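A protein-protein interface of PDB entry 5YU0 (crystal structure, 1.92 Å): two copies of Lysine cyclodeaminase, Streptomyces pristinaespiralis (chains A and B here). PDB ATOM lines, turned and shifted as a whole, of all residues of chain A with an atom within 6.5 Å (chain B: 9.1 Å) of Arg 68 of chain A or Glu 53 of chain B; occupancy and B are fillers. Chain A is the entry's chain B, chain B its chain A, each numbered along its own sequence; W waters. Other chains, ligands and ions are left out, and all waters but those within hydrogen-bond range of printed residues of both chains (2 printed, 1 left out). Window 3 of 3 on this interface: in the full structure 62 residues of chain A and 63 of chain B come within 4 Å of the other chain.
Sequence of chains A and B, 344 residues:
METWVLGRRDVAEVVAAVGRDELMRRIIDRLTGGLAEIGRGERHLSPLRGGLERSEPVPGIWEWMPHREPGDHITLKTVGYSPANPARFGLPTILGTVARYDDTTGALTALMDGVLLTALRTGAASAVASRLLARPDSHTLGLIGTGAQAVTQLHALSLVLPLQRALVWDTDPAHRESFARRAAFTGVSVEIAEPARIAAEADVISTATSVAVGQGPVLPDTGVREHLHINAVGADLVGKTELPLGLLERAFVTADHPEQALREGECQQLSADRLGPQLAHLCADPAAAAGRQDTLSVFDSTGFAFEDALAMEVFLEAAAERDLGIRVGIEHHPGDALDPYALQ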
ATOM      1  N   HIS A  44      -2.516 -24.222 -34.949  1.00  0.00           N
ATOM      2  CA  HIS A  44      -2.678 -22.809 -34.652  1.00  0.00           C
ATOM      3  C   HIS A  44      -1.367 -22.066 -34.837  1.00  0.00           C
ATOM      4  O   HIS A  44      -0.279 -22.635 -34.685  1.00  0.00           O
ATOM      5  CB  HIS A  44      -3.239 -22.634 -33.241  1.00  0.00           C
ATOM      6  CG  HIS A  44      -4.502 -23.406 -33.023  1.00  0.00           C
ATOM      7  ND1 HIS A  44      -5.740 -22.928 -33.401  1.00  0.00           N
ATOM      8  CD2 HIS A  44      -4.715 -24.646 -32.520  1.00  0.00           C
ATOM      9  CE1 HIS A  44      -6.664 -23.827 -33.114  1.00  0.00           C
ATOM     10  NE2 HIS A  44      -6.069 -24.879 -32.579  1.00  0.00           N
ATOM     11  N   SER A  46       1.763 -19.925 -34.155  1.00  0.00           N
ATOM     12  CA  SER A  46       2.624 -19.750 -33.000  1.00  0.00           C
ATOM     13  C   SER A  46       2.346 -18.401 -32.344  1.00  0.00           C
ATOM     14  O   SER A  46       1.850 -17.472 -32.989  1.00  0.00           O
ATOM     15  CB  SER A  46       4.103 -19.835 -33.410  1.00  0.00           C
ATOM     16  OG  SER A  46       4.310 -20.823 -34.415  1.00  0.00           O
ATOM     17  N   PRO A  47       2.641 -18.273 -31.053  1.00  0.00           N
ATOM     18  CA  PRO A  47       2.572 -16.955 -30.416  1.00  0.00           C
ATOM     19  C   PRO A  47       3.585 -15.995 -31.023  1.00  0.00           C
ATOM     20  O   PRO A  47       4.567 -16.394 -31.659  1.00  0.00           O
ATOM     21  CB  PRO A  47       2.900 -17.249 -28.947  1.00  0.00           C
ATOM     22  CG  PRO A  47       3.640 -18.531 -28.977  1.00  0.00           C
ATOM     23  CD  PRO A  47       3.024 -19.321 -30.097  1.00  0.00           C
ATOM     24  N   PRO A  66       8.857 -19.400 -29.664  1.00  0.00           N
ATOM     25  CA  PRO A  66       8.330 -20.695 -29.220  1.00  0.00           C
ATOM     26  C   PRO A  66       7.169 -21.182 -30.074  1.00  0.00           C
ATOM     27  O   PRO A  66       6.429 -20.403 -30.683  1.00  0.00           O
ATOM     28  CB  PRO A  66       7.857 -20.392 -27.788  1.00  0.00           C
ATOM     29  CG  PRO A  66       7.435 -18.957 -27.848  1.00  0.00           C
ATOM     30  CD  PRO A  66       8.416 -18.291 -28.792  1.00  0.00           C
ATOM     31  N   HIS A  67       7.024 -22.504 -30.122  1.00  0.00           N
ATOM     32  CA  HIS A  67       5.848 -23.124 -30.718  1.00  0.00           C
ATOM     33  C   HIS A  67       5.546 -24.434 -30.002  1.00  0.00           C
ATOM     34  O   HIS A  67       6.449 -25.240 -29.753  1.00  0.00           O
ATOM     35  CB  HIS A  67       6.002 -23.408 -32.215  1.00  0.00           C
ATOM     36  CG  HIS A  67       4.791 -24.060 -32.808  1.00  0.00           C
ATOM     37  ND1 HIS A  67       3.721 -23.337 -33.294  1.00  0.00           N
ATOM     38  CD2 HIS A  67       4.454 -25.366 -32.939  1.00  0.00           C
ATOM     39  CE1 HIS A  67       2.785 -24.170 -33.715  1.00  0.00           C
ATOM     40  NE2 HIS A  67       3.202 -25.406 -33.506  1.00  0.00           N
ATOM     41  N   ARG A  68       4.266 -24.657 -29.717  1.00  0.00           N
ATOM     42  CA  ARG A  68       3.822 -25.807 -28.942  1.00  0.00           C
ATOM     43  C   ARG A  68       2.966 -26.727 -29.801  1.00  0.00           C
ATOM     44  O   ARG A  68       1.984 -26.282 -30.409  1.00  0.00           O
ATOM     45  CB  ARG A  68       3.010 -25.372 -27.719  1.00  0.00           C
ATOM     46  CG  ARG A  68       2.331 -26.530 -27.012  1.00  0.00           C
ATOM     47  CD  ARG A  68       1.912 -26.137 -25.610  1.00  0.00           C
ATOM     48  NE  ARG A  68       1.413 -27.295 -24.874  1.00  0.00           N
ATOM     49  CZ  ARG A  68       0.133 -27.524 -24.620  1.00  0.00           C
ATOM     50  NH1 ARG A  68      -0.786 -26.659 -25.038  1.00  0.00           N
ATOM     51  NH2 ARG A  68      -0.226 -28.618 -23.948  1.00  0.00           N
ATOM     52  N   GLU A  69       3.329 -28.009 -29.828  1.00  0.00           N
ATOM     53  CA  GLU A  69       2.444 -29.040 -30.363  1.00  0.00           C
ATOM     54  C   GLU A  69       1.879 -29.822 -29.183  1.00  0.00           C
ATOM     55  O   GLU A  69       2.564 -30.702 -28.634  1.00  0.00           O
ATOM     56  CB  GLU A  69       3.180 -29.958 -31.338  1.00  0.00           C
ATOM     57  CG  GLU A  69       3.483 -29.272 -32.687  1.00  0.00           C
ATOM     58  CD  GLU A  69       2.232 -29.071 -33.540  1.00  0.00           C
ATOM     59  OE1 GLU A  69       1.544 -30.078 -33.820  1.00  0.00           O
ATOM     60  OE2 GLU A  69       1.927 -27.913 -33.928  1.00  0.00           O
ATOM     61  N   PRO A  70       0.650 -29.534 -28.762  1.00  0.00           N
ATOM     62  CA  PRO A  70       0.155 -30.026 -27.467  1.00  0.00           C
ATOM     63  C   PRO A  70       0.210 -31.545 -27.360  1.00  0.00           C
ATOM     64  O   PRO A  70      -0.174 -32.267 -28.283  1.00  0.00           O
ATOM     65  CB  PRO A  70      -1.284 -29.505 -27.421  1.00  0.00           C
ATOM     66  CG  PRO A  70      -1.286 -28.311 -28.348  1.00  0.00           C
ATOM     67  CD  PRO A  70      -0.315 -28.653 -29.440  1.00  0.00           C
ATOM     68  N   GLY A  71       0.713 -32.022 -26.216  1.00  0.00           N
ATOM     69  CA  GLY A  71       0.900 -33.435 -25.968  1.00  0.00           C
ATOM     70  C   GLY A  71       2.121 -34.042 -26.618  1.00  0.00           C
ATOM     71  O   GLY A  71       2.483 -35.176 -26.276  1.00  0.00           O
ATOM     72  N   HIS A  73       5.452 -31.909 -28.278  1.00  0.00           N
ATOM     73  CA  HIS A  73       6.668 -31.204 -27.932  1.00  0.00           C
ATOM     74  C   HIS A  73       6.495 -29.707 -28.114  1.00  0.00           C
ATOM     75  O   HIS A  73       5.551 -29.226 -28.749  1.00  0.00           O
ATOM     76  CB  HIS A  73       7.852 -31.699 -28.763  1.00  0.00           C
ATOM     77  CG  HIS A  73       7.535 -31.853 -30.212  1.00  0.00           C
ATOM     78  ND1 HIS A  73       7.432 -30.776 -31.065  1.00  0.00           N
ATOM     79  CD2 HIS A  73       7.282 -32.954 -30.958  1.00  0.00           C
ATOM     80  CE1 HIS A  73       7.140 -31.209 -32.280  1.00  0.00           C
ATOM     81  NE2 HIS A  73       7.041 -32.526 -32.241  1.00  0.00           N
ATOM     82  N   ILE A  74       7.435 -28.990 -27.521  1.00  0.00           N
ATOM     83  CA  ILE A  74       7.565 -27.547 -27.640  1.00  0.00           C
ATOM     84  C   ILE A  74       8.860 -27.282 -28.387  1.00  0.00           C
ATOM     85  O   ILE A  74       9.893 -27.891 -28.084  1.00  0.00           O
ATOM     86  CB  ILE A  74       7.574 -26.878 -26.253  1.00  0.00           C
ATOM     87  CG1 ILE A  74       6.257 -27.158 -25.533  1.00  0.00           C
ATOM     88  CG2 ILE A  74       7.840 -25.373 -26.353  1.00  0.00           C
ATOM     89  CD1 ILE A  74       6.155 -26.473 -24.189  1.00  0.00           C
ATOM     90  N   THR A  75       8.796 -26.415 -29.387  1.00  0.00           N
ATOM     91  CA  THR A  75       9.970 -25.976 -30.121  1.00  0.00           C
ATOM     92  C   THR A  75      10.286 -24.547 -29.717  1.00  0.00           C
ATOM     93  O   THR A  75       9.377 -23.725 -29.570  1.00  0.00           O
ATOM     94  CB  THR A  75       9.734 -26.047 -31.637  1.00  0.00           C
ATOM     95  OG1 THR A  75       9.392 -27.383 -32.006  1.00  0.00           O
ATOM     96  CG2 THR A  75      10.994 -25.639 -32.390  1.00  0.00           C
ATOM     97  N   ASP A 103       6.556 -32.063 -24.359  1.00  0.00           N
ATOM     98  CA  ASP A 103       5.459 -31.247 -23.846  1.00  0.00           C
ATOM     99  C   ASP A 103       4.886 -31.810 -22.552  1.00  0.00           C
ATOM    100  O   ASP A 103       4.385 -31.048 -21.719  1.00  0.00           O
ATOM    101  CB  ASP A 103       4.352 -31.115 -24.888  1.00  0.00           C
ATOM    102  CG  ASP A 103       3.278 -30.142 -24.452  1.00  0.00           C
ATOM    103  OD1 ASP A 103       3.625 -28.961 -24.218  1.00  0.00           O
ATOM    104  OD2 ASP A 103       2.104 -30.563 -24.323  1.00  0.00           O
ATOM    105  N   GLY B  50       7.511 -15.020 -20.492  1.00  0.00           N
ATOM    106  CA  GLY B  50       6.362 -15.528 -21.208  1.00  0.00           C
ATOM    107  C   GLY B  50       6.216 -17.019 -20.949  1.00  0.00           C
ATOM    108  O   GLY B  50       7.102 -17.662 -20.370  1.00  0.00           O
ATOM    109  N   GLY B  51       5.086 -17.570 -21.376  1.00  0.00           N
ATOM    110  CA  GLY B  51       4.842 -18.972 -21.115  1.00  0.00           C
ATOM    111  C   GLY B  51       3.726 -19.552 -21.951  1.00  0.00           C
ATOM    112  O   GLY B  51       2.901 -18.831 -22.528  1.00  0.00           O
ATOM    113  N   LEU B  52       3.716 -20.882 -22.002  1.00  0.00           N
ATOM    114  CA  LEU B  52       2.697 -21.682 -22.672  1.00  0.00           C
ATOM    115  C   LEU B  52       2.046 -22.597 -21.645  1.00  0.00           C
ATOM    116  O   LEU B  52       2.715 -23.476 -21.085  1.00  0.00           O
ATOM    117  CB  LEU B  52       3.307 -22.523 -23.801  1.00  0.00           C
ATOM    118  CG  LEU B  52       3.852 -21.814 -25.049  1.00  0.00           C
ATOM    119  CD1 LEU B  52       5.056 -22.548 -25.614  1.00  0.00           C
ATOM    120  CD2 LEU B  52       2.760 -21.743 -26.087  1.00  0.00           C
ATOM    121  N   GLU B  53       0.740 -22.435 -21.439  1.00  0.00           N
ATOM    122  CA  GLU B  53       0.005 -23.300 -20.524  1.00  0.00           C
ATOM    123  C   GLU B  53      -0.184 -24.693 -21.114  1.00  0.00           C
ATOM    124  O   GLU B  53      -0.379 -24.854 -22.320  1.00  0.00           O
ATOM    125  CB  GLU B  53      -1.361 -22.698 -20.199  1.00  0.00           C
ATOM    126  CG  GLU B  53      -1.286 -21.406 -19.401  1.00  0.00           C
ATOM    127  CD  GLU B  53      -2.640 -21.008 -18.842  1.00  0.00           C
ATOM    128  OE1 GLU B  53      -2.693 -20.079 -18.004  1.00  0.00           O
ATOM    129  OE2 GLU B  53      -3.646 -21.637 -19.240  1.00  0.00           O
ATOM    130  N   ARG B  54      -0.122 -25.705 -20.250  1.00  0.00           N
ATOM    131  CA  ARG B  54      -0.304 -27.098 -20.641  1.00  0.00           C
ATOM    132  C   ARG B  54      -1.320 -27.718 -19.694  1.00  0.00           C
ATOM    133  O   ARG B  54      -1.220 -27.548 -18.475  1.00  0.00           O
ATOM    134  CB  ARG B  54       1.034 -27.867 -20.608  1.00  0.00           C
ATOM    135  CG  ARG B  54       2.089 -27.364 -21.613  1.00  0.00           C
ATOM    136  CD  ARG B  54       3.489 -27.951 -21.328  1.00  0.00           C
ATOM    137  NE  ARG B  54       3.850 -27.626 -19.975  1.00  0.00           N
ATOM    138  CZ  ARG B  54       4.507 -28.404 -19.124  1.00  0.00           C
ATOM    139  NH1 ARG B  54       4.954 -29.617 -19.452  1.00  0.00           N
ATOM    140  NH2 ARG B  54       4.710 -27.934 -17.915  1.00  0.00           N
ATOM    141  N   SER B  55      -2.308 -28.419 -20.240  1.00  0.00           N
ATOM    142  CA  SER B  55      -3.386 -28.910 -19.391  1.00  0.00           C
ATOM    143  C   SER B  55      -3.196 -30.343 -18.923  1.00  0.00           C
ATOM    144  O   SER B  55      -3.755 -30.713 -17.889  1.00  0.00           O
ATOM    145  CB  SER B  55      -4.730 -28.793 -20.118  1.00  0.00           C
ATOM    146  OG  SER B  55      -4.684 -29.482 -21.349  1.00  0.00           O
ATOM    147  N   GLU B  56      -2.419 -31.152 -19.634  1.00  0.00           N
ATOM    148  CA  GLU B  56      -2.309 -32.560 -19.293  1.00  0.00           C
ATOM    149  C   GLU B  56      -0.884 -32.914 -18.874  1.00  0.00           C
ATOM    150  O   GLU B  56       0.076 -32.331 -19.382  1.00  0.00           O
ATOM    151  CB  GLU B  56      -2.727 -33.433 -20.484  1.00  0.00           C
ATOM    152  CG  GLU B  56      -4.212 -33.331 -20.800  1.00  0.00           C
ATOM    153  CD  GLU B  56      -4.631 -34.253 -21.927  1.00  0.00           C
ATOM    154  OE1 GLU B  56      -3.768 -35.001 -22.435  1.00  0.00           O
ATOM    155  OE2 GLU B  56      -5.826 -34.240 -22.296  1.00  0.00           O
ATOM    156  N   PRO B  57      -0.709 -33.887 -17.960  1.00  0.00           N
ATOM    157  CA  PRO B  57      -1.748 -34.664 -17.275  1.00  0.00           C
ATOM    158  C   PRO B  57      -2.471 -33.849 -16.206  1.00  0.00           C
ATOM    159  O   PRO B  57      -3.609 -34.151 -15.863  1.00  0.00           O
ATOM    160  CB  PRO B  57      -0.961 -35.827 -16.648  1.00  0.00           C
ATOM    161  CG  PRO B  57       0.406 -35.315 -16.493  1.00  0.00           C
ATOM    162  CD  PRO B  57       0.644 -34.369 -17.630  1.00  0.00           C
ATOM    163  N   VAL B  58      -1.794 -32.832 -15.683  1.00  0.00           N
ATOM    164  CA  VAL B  58      -2.408 -31.815 -14.828  1.00  0.00           C
ATOM    165  C   VAL B  58      -1.937 -30.460 -15.333  1.00  0.00           C
ATOM    166  O   VAL B  58      -0.954 -30.379 -16.085  1.00  0.00           O
ATOM    167  CB  VAL B  58      -2.036 -32.014 -13.341  1.00  0.00           C
ATOM    168  CG1 VAL B  58      -2.426 -33.409 -12.863  1.00  0.00           C
ATOM    169  CG2 VAL B  58      -0.552 -31.783 -13.154  1.00  0.00           C
ATOM    170  N   PRO B  59      -2.627 -29.378 -14.967  1.00  0.00           N
ATOM    171  CA  PRO B  59      -2.231 -28.059 -15.477  1.00  0.00           C
ATOM    172  C   PRO B  59      -0.808 -27.694 -15.079  1.00  0.00           C
ATOM    173  O   PRO B  59      -0.426 -27.775 -13.908  1.00  0.00           O
ATOM    174  CB  PRO B  59      -3.252 -27.112 -14.841  1.00  0.00           C
ATOM    175  CG  PRO B  59      -4.479 -27.986 -14.663  1.00  0.00           C
ATOM    176  CD  PRO B  59      -3.917 -29.321 -14.251  1.00  0.00           C
ATOM    177  N   GLY B  60      -0.029 -27.290 -16.071  1.00  0.00           N
ATOM    178  CA  GLY B  60       1.327 -26.837 -15.845  1.00  0.00           C
ATOM    179  C   GLY B  60       1.633 -25.728 -16.824  1.00  0.00           C
ATOM    180  O   GLY B  60       0.735 -25.279 -17.546  1.00  0.00           O
ATOM    181  N   ILE B  61       2.882 -25.273 -16.861  1.00  0.00           N
ATOM    182  CA  ILE B  61       3.273 -24.195 -17.759  1.00  0.00           C
ATOM    183  C   ILE B  61       4.733 -24.396 -18.142  1.00  0.00           C
ATOM    184  O   ILE B  61       5.507 -25.014 -17.407  1.00  0.00           O
ATOM    185  CB  ILE B  61       3.028 -22.804 -17.109  1.00  0.00           C
ATOM    186  CG1 ILE B  61       3.063 -21.685 -18.168  1.00  0.00           C
ATOM    187  CG2 ILE B  61       4.033 -22.539 -15.981  1.00  0.00           C
ATOM    188  CD1 ILE B  61       2.502 -20.339 -17.674  1.00  0.00           C
ATOM    189  N   TRP B  62       5.101 -23.898 -19.319  1.00  0.00           N
ATOM    190  CA  TRP B  62       6.489 -23.906 -19.771  1.00  0.00           C
ATOM    191  C   TRP B  62       6.832 -22.482 -20.174  1.00  0.00           C
ATOM    192  O   TRP B  62       6.085 -21.862 -20.943  1.00  0.00           O
ATOM    193  CB  TRP B  62       6.694 -24.890 -20.935  1.00  0.00           C
ATOM    194  CG  TRP B  62       8.113 -25.014 -21.356  1.00  0.00           C
ATOM    195  CD1 TRP B  62       9.059 -25.848 -20.823  1.00  0.00           C
ATOM    196  CD2 TRP B  62       8.768 -24.268 -22.386  1.00  0.00           C
ATOM    197  NE1 TRP B  62      10.259 -25.668 -21.469  1.00  0.00           N
ATOM    198  CE2 TRP B  62      10.107 -24.702 -22.430  1.00  0.00           C
ATOM    199  CE3 TRP B  62       8.349 -23.278 -23.282  1.00  0.00           C
ATOM    200  CZ2 TRP B  62      11.033 -24.180 -23.333  1.00  0.00           C
ATOM    201  CZ3 TRP B  62       9.271 -22.763 -24.175  1.00  0.00           C
ATOM    202  CH2 TRP B  62      10.595 -23.212 -24.192  1.00  0.00           C
ATOM    203  N   GLU B  63       7.925 -21.948 -19.618  1.00  0.00           N
ATOM    204  CA  GLU B  63       8.180 -20.515 -19.644  1.00  0.00           C
ATOM    205  C   GLU B  63       9.585 -20.211 -20.142  1.00  0.00           C
ATOM    206  O   GLU B  63      10.510 -21.018 -19.997  1.00  0.00           O
ATOM    207  CB  GLU B  63       7.985 -19.884 -18.241  1.00  0.00           C
ATOM    208  CG  GLU B  63       6.547 -19.997 -17.743  1.00  0.00           C
ATOM    209  CD  GLU B  63       6.353 -19.552 -16.288  1.00  0.00           C
ATOM    210  OE1 GLU B  63       7.194 -19.886 -15.432  1.00  0.00           O
ATOM    211  OE2 GLU B  63       5.345 -18.875 -16.006  1.00  0.00           O
ATOM    212  N   TRP B  64       9.737 -19.014 -20.710  1.00  0.00           N
ATOM    213  CA  TRP B  64      11.025 -18.528 -21.190  1.00  0.00           C
ATOM    214  C   TRP B  64      11.296 -17.175 -20.553  1.00  0.00           C
ATOM    215  O   TRP B  64      10.371 -16.388 -20.345  1.00  0.00           O
ATOM    216  CB  TRP B  64      11.063 -18.421 -22.726  1.00  0.00           C
ATOM    217  CG  TRP B  64       9.896 -17.653 -23.313  1.00  0.00           C
ATOM    218  CD1 TRP B  64       9.854 -16.322 -23.606  1.00  0.00           C
ATOM    219  CD2 TRP B  64       8.609 -18.182 -23.663  1.00  0.00           C
ATOM    220  NE1 TRP B  64       8.618 -15.986 -24.119  1.00  0.00           N
ATOM    221  CE2 TRP B  64       7.838 -17.110 -24.168  1.00  0.00           C
ATOM    222  CE3 TRP B  64       8.032 -19.458 -23.596  1.00  0.00           C
ATOM    223  CZ2 TRP B  64       6.520 -17.274 -24.608  1.00  0.00           C
ATOM    224  CZ3 TRP B  64       6.721 -19.619 -24.040  1.00  0.00           C
ATOM    225  CH2 TRP B  64       5.983 -18.530 -24.538  1.00  0.00           C
ATOM    226  N   TYR B  81       7.084 -26.180 -15.587  1.00  0.00           N
ATOM    227  CA  TYR B  81       6.414 -26.519 -14.337  1.00  0.00           C
ATOM    228  C   TYR B  81       5.394 -27.591 -14.678  1.00  0.00           C
ATOM    229  O   TYR B  81       4.431 -27.326 -15.415  1.00  0.00           O
ATOM    230  CB  TYR B  81       5.747 -25.292 -13.713  1.00  0.00           C
ATOM    231  CG  TYR B  81       4.720 -25.615 -12.646  1.00  0.00           C
ATOM    232  CD1 TYR B  81       5.115 -25.960 -11.353  1.00  0.00           C
ATOM    233  CD2 TYR B  81       3.354 -25.556 -12.926  1.00  0.00           C
ATOM    234  CE1 TYR B  81       4.153 -26.248 -10.349  1.00  0.00           C
ATOM    235  CE2 TYR B  81       2.394 -25.832 -11.942  1.00  0.00           C
ATOM    236  CZ  TYR B  81       2.802 -26.169 -10.652  1.00  0.00           C
ATOM    237  OH  TYR B  81       1.855 -26.438  -9.675  1.00  0.00           O
ATOM    238  N   VAL B 213      -4.535 -23.570  -9.507  1.00  0.00           N
ATOM    239  CA  VAL B 213      -5.233 -22.294  -9.624  1.00  0.00           C
ATOM    240  C   VAL B 213      -6.557 -22.357  -8.876  1.00  0.00           C
ATOM    241  O   VAL B 213      -7.336 -23.302  -9.046  1.00  0.00           O
ATOM    242  CB  VAL B 213      -5.455 -21.956 -11.113  1.00  0.00           C
ATOM    243  CG1 VAL B 213      -6.455 -20.801 -11.277  1.00  0.00           C
ATOM    244  CG2 VAL B 213      -4.130 -21.628 -11.791  1.00  0.00           C
ATOM    245  N   ASP B 236       3.359 -20.171 -10.901  1.00  0.00           N
ATOM    246  CA  ASP B 236       3.365 -20.856 -12.184  1.00  0.00           C
ATOM    247  C   ASP B 236       2.309 -20.250 -13.105  1.00  0.00           C
ATOM    248  O   ASP B 236       2.627 -19.401 -13.947  1.00  0.00           O
ATOM    249  CB  ASP B 236       3.144 -22.360 -11.994  1.00  0.00           C
ATOM    250  CG  ASP B 236       2.053 -22.685 -10.952  1.00  0.00           C
ATOM    251  OD1 ASP B 236       0.871 -22.771 -11.342  1.00  0.00           O
ATOM    252  OD2 ASP B 236       2.386 -22.912  -9.762  1.00  0.00           O
ATOM    253  N   LEU B 237       1.056 -20.660 -12.932  1.00  0.00           N
ATOM    254  CA  LEU B 237      -0.048 -20.203 -13.764  1.00  0.00           C
ATOM    255  C   LEU B 237      -0.653 -18.912 -13.221  1.00  0.00           C
ATOM    256  O   LEU B 237      -0.701 -18.685 -12.009  1.00  0.00           O
ATOM    257  CB  LEU B 237      -1.135 -21.278 -13.832  1.00  0.00           C
ATOM    258  CG  LEU B 237      -0.721 -22.606 -14.468  1.00  0.00           C
ATOM    259  CD1 LEU B 237      -1.596 -23.743 -13.976  1.00  0.00           C
ATOM    260  CD2 LEU B 237      -0.803 -22.487 -15.971  1.00  0.00           C
ATOM    261  N   VAL B 238      -1.143 -18.067 -14.136  1.00  0.00           N
ATOM    262  CA  VAL B 238      -2.022 -16.977 -13.723  1.00  0.00           C
ATOM    263  C   VAL B 238      -3.196 -17.559 -12.955  1.00  0.00           C
ATOM    264  O   VAL B 238      -3.807 -18.549 -13.377  1.00  0.00           O
ATOM    265  CB  VAL B 238      -2.495 -16.177 -14.949  1.00  0.00           C
ATOM    266  CG1 VAL B 238      -3.630 -15.226 -14.567  1.00  0.00           C
ATOM    267  CG2 VAL B 238      -1.337 -15.418 -15.552  1.00  0.00           C
ATOM    268  N   GLY B 239      -3.505 -16.962 -11.804  1.00  0.00           N
ATOM    269  CA  GLY B 239      -4.569 -17.440 -10.952  1.00  0.00           C
ATOM    270  C   GLY B 239      -4.109 -18.271  -9.771  1.00  0.00           C
ATOM    271  O   GLY B 239      -4.920 -18.538  -8.876  1.00  0.00           O
ATOM    272  N   LYS B 240      -2.838 -18.678  -9.737  1.00  0.00           N
ATOM    273  CA  LYS B 240      -2.308 -19.493  -8.651  1.00  0.00           C
ATOM    274  C   LYS B 240      -1.809 -18.573  -7.547  1.00  0.00           C
ATOM    275  O   LYS B 240      -0.931 -17.736  -7.781  1.00  0.00           O
ATOM    276  CB  LYS B 240      -1.187 -20.411  -9.149  1.00  0.00           C
ATOM    277  CG  LYS B 240      -0.577 -21.347  -8.073  1.00  0.00           C
ATOM    278  CD  LYS B 240       0.901 -21.037  -7.847  1.00  0.00           C
ATOM    279  CE  LYS B 240       1.552 -22.004  -6.853  1.00  0.00           C
ATOM    280  NZ  LYS B 240       1.426 -23.424  -7.285  1.00  0.00           N
ATOM    281  N   ARG B 263       1.002 -10.218 -11.990  1.00  0.00           N
ATOM    282  CA  ARG B 263       0.427 -11.202 -12.901  1.00  0.00           C
ATOM    283  C   ARG B 263       0.438 -12.619 -12.336  1.00  0.00           C
ATOM    284  O   ARG B 263      -0.523 -13.377 -12.545  1.00  0.00           O
ATOM    285  CB  ARG B 263       1.200 -11.169 -14.220  1.00  0.00           C
ATOM    286  CG  ARG B 263       0.633 -12.047 -15.308  1.00  0.00           C
ATOM    287  CD  ARG B 263       1.065 -11.558 -16.672  1.00  0.00           C
ATOM    288  NE  ARG B 263       2.498 -11.760 -16.867  1.00  0.00           N
ATOM    289  CZ  ARG B 263       3.062 -12.919 -17.211  1.00  0.00           C
ATOM    290  NH1 ARG B 263       2.317 -13.998 -17.398  1.00  0.00           N
ATOM    291  NH2 ARG B 263       4.376 -13.016 -17.372  1.00  0.00           N
ATOM    292  N   GLU B 264       1.520 -13.000 -11.636  1.00  0.00           N
ATOM    293  CA  GLU B 264       1.751 -14.388 -11.260  1.00  0.00           C
ATOM    294  C   GLU B 264       2.077 -14.613  -9.792  1.00  0.00           C
ATOM    295  O   GLU B 264       2.167 -15.779  -9.387  1.00  0.00           O
ATOM    296  CB  GLU B 264       2.892 -14.997 -12.101  1.00  0.00           C
ATOM    297  CG  GLU B 264       2.519 -15.222 -13.567  1.00  0.00           C
ATOM    298  CD  GLU B 264       3.693 -15.725 -14.418  1.00  0.00           C
ATOM    299  OE1 GLU B 264       4.338 -16.734 -14.046  1.00  0.00           O
ATOM    300  OE2 GLU B 264       3.969 -15.110 -15.467  1.00  0.00           O
HETATM  301  O   HOH W   1       1.245 -31.614 -22.024  1.00  0.00           O
HETATM  302  O   HOH W   2       2.342 -31.100 -18.951  1.00  0.00           O
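Hydrophobic or aromatic side chains of chain A within 4 Å of the printed part of chain B: Pro 66 and Ile 74.
Along chain A the printed residues that touch a printed residue of chain B span positions 66 to 103.
No position is printed for both chains.
Of the 6 pairs that touch across the chains among the printed residues, none has its exchanged pair printed and touching as well.
Printed residues of chain A within 4 Å of Glu 53 of chain B: Arg 68.
No residue of chain B comes within 4 Å of His 67 of chain A.
Of the printed residues of chain A, Arg 54 of chain B touches Arg 68 and Asp 103.
Printed residues of chain B within 4 Å of Pro 66 of chain A: Trp 64.
Printed residues of chain A within 4 Å of Trp 62 of chain B: Ile 74.
Of the printed residues of chain B, Asp 103 of chain A touches Arg 54 (2.7 Å).
The nearest printed residue of chain B that does not touch Arg 68 of chain A is Ser 55 of chain B (4.3 Å).
The nearest printed residue of chain A that does not touch Trp 62 of chain B is Pro 66 of chain A (4.5 Å).
Among the printed residues, merely in contact across the chains: Arg 68 of chain A with Arg 54 of chain B, Pro 66 of chain A with Trp 64 of chain B, Ile 74 of chain A with Trp 62 of chain B and Arg 68 of chain A with Leu 52 of chain B.
The backbone carbonyl oxygen (O) of Glu 53 of chain B is in hydrogen-bond range of the guanidinium group (NH1) of Arg 68 of chain A (3.3 Å).
The backbone carbonyl oxygen of Asp 103 of chain A sits at hydrogen-bond distance from the guanidinium group of Arg 54 of chain B (2.7 Å).
O of Gly 50 of chain B lies within hydrogen-bond range of N of Trp 64 of chain B (3.0 Å).
The backbone NH of Gly 60 of chain B is in hydrogen-bond range of the backbone carbonyl oxygen of Arg 54 of chain B (2.7 Å).
The guanidinium group (NH2) of Arg 54 of chain B sits at hydrogen-bond distance from the backbone carbonyl oxygen (O) of Ile 61 of chain B (3.1 Å).
NH2 of Arg 54 of chain B sits at hydrogen-bond distance from O of Tyr 81 of chain B (2.6 Å).
NE of Arg 68 of chain A lies within salt-bridge range of OD1 of Asp 103 of chain A (2.8 Å).
The backbone NH of Gly 71 of chain A is in hydrogen-bond range of the side-chain carboxylate of Asp 103 of chain A (2.8 Å).
Water W2 lies within hydrogen-bond range of the backbone carbonyl oxygen (O) of Glu 56 of chain B (2.6 Å), the guanidinium group (NH1) of Arg 54 of chain B (3.0 Å) and the backbone carbonyl oxygen (O) of Asp 103 of chain A (3.4 Å).
Water W1 bridges OD2 of Asp 103 of chain A (2.7 Å) and O of Glu 56 of chain B (3.0 Å).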
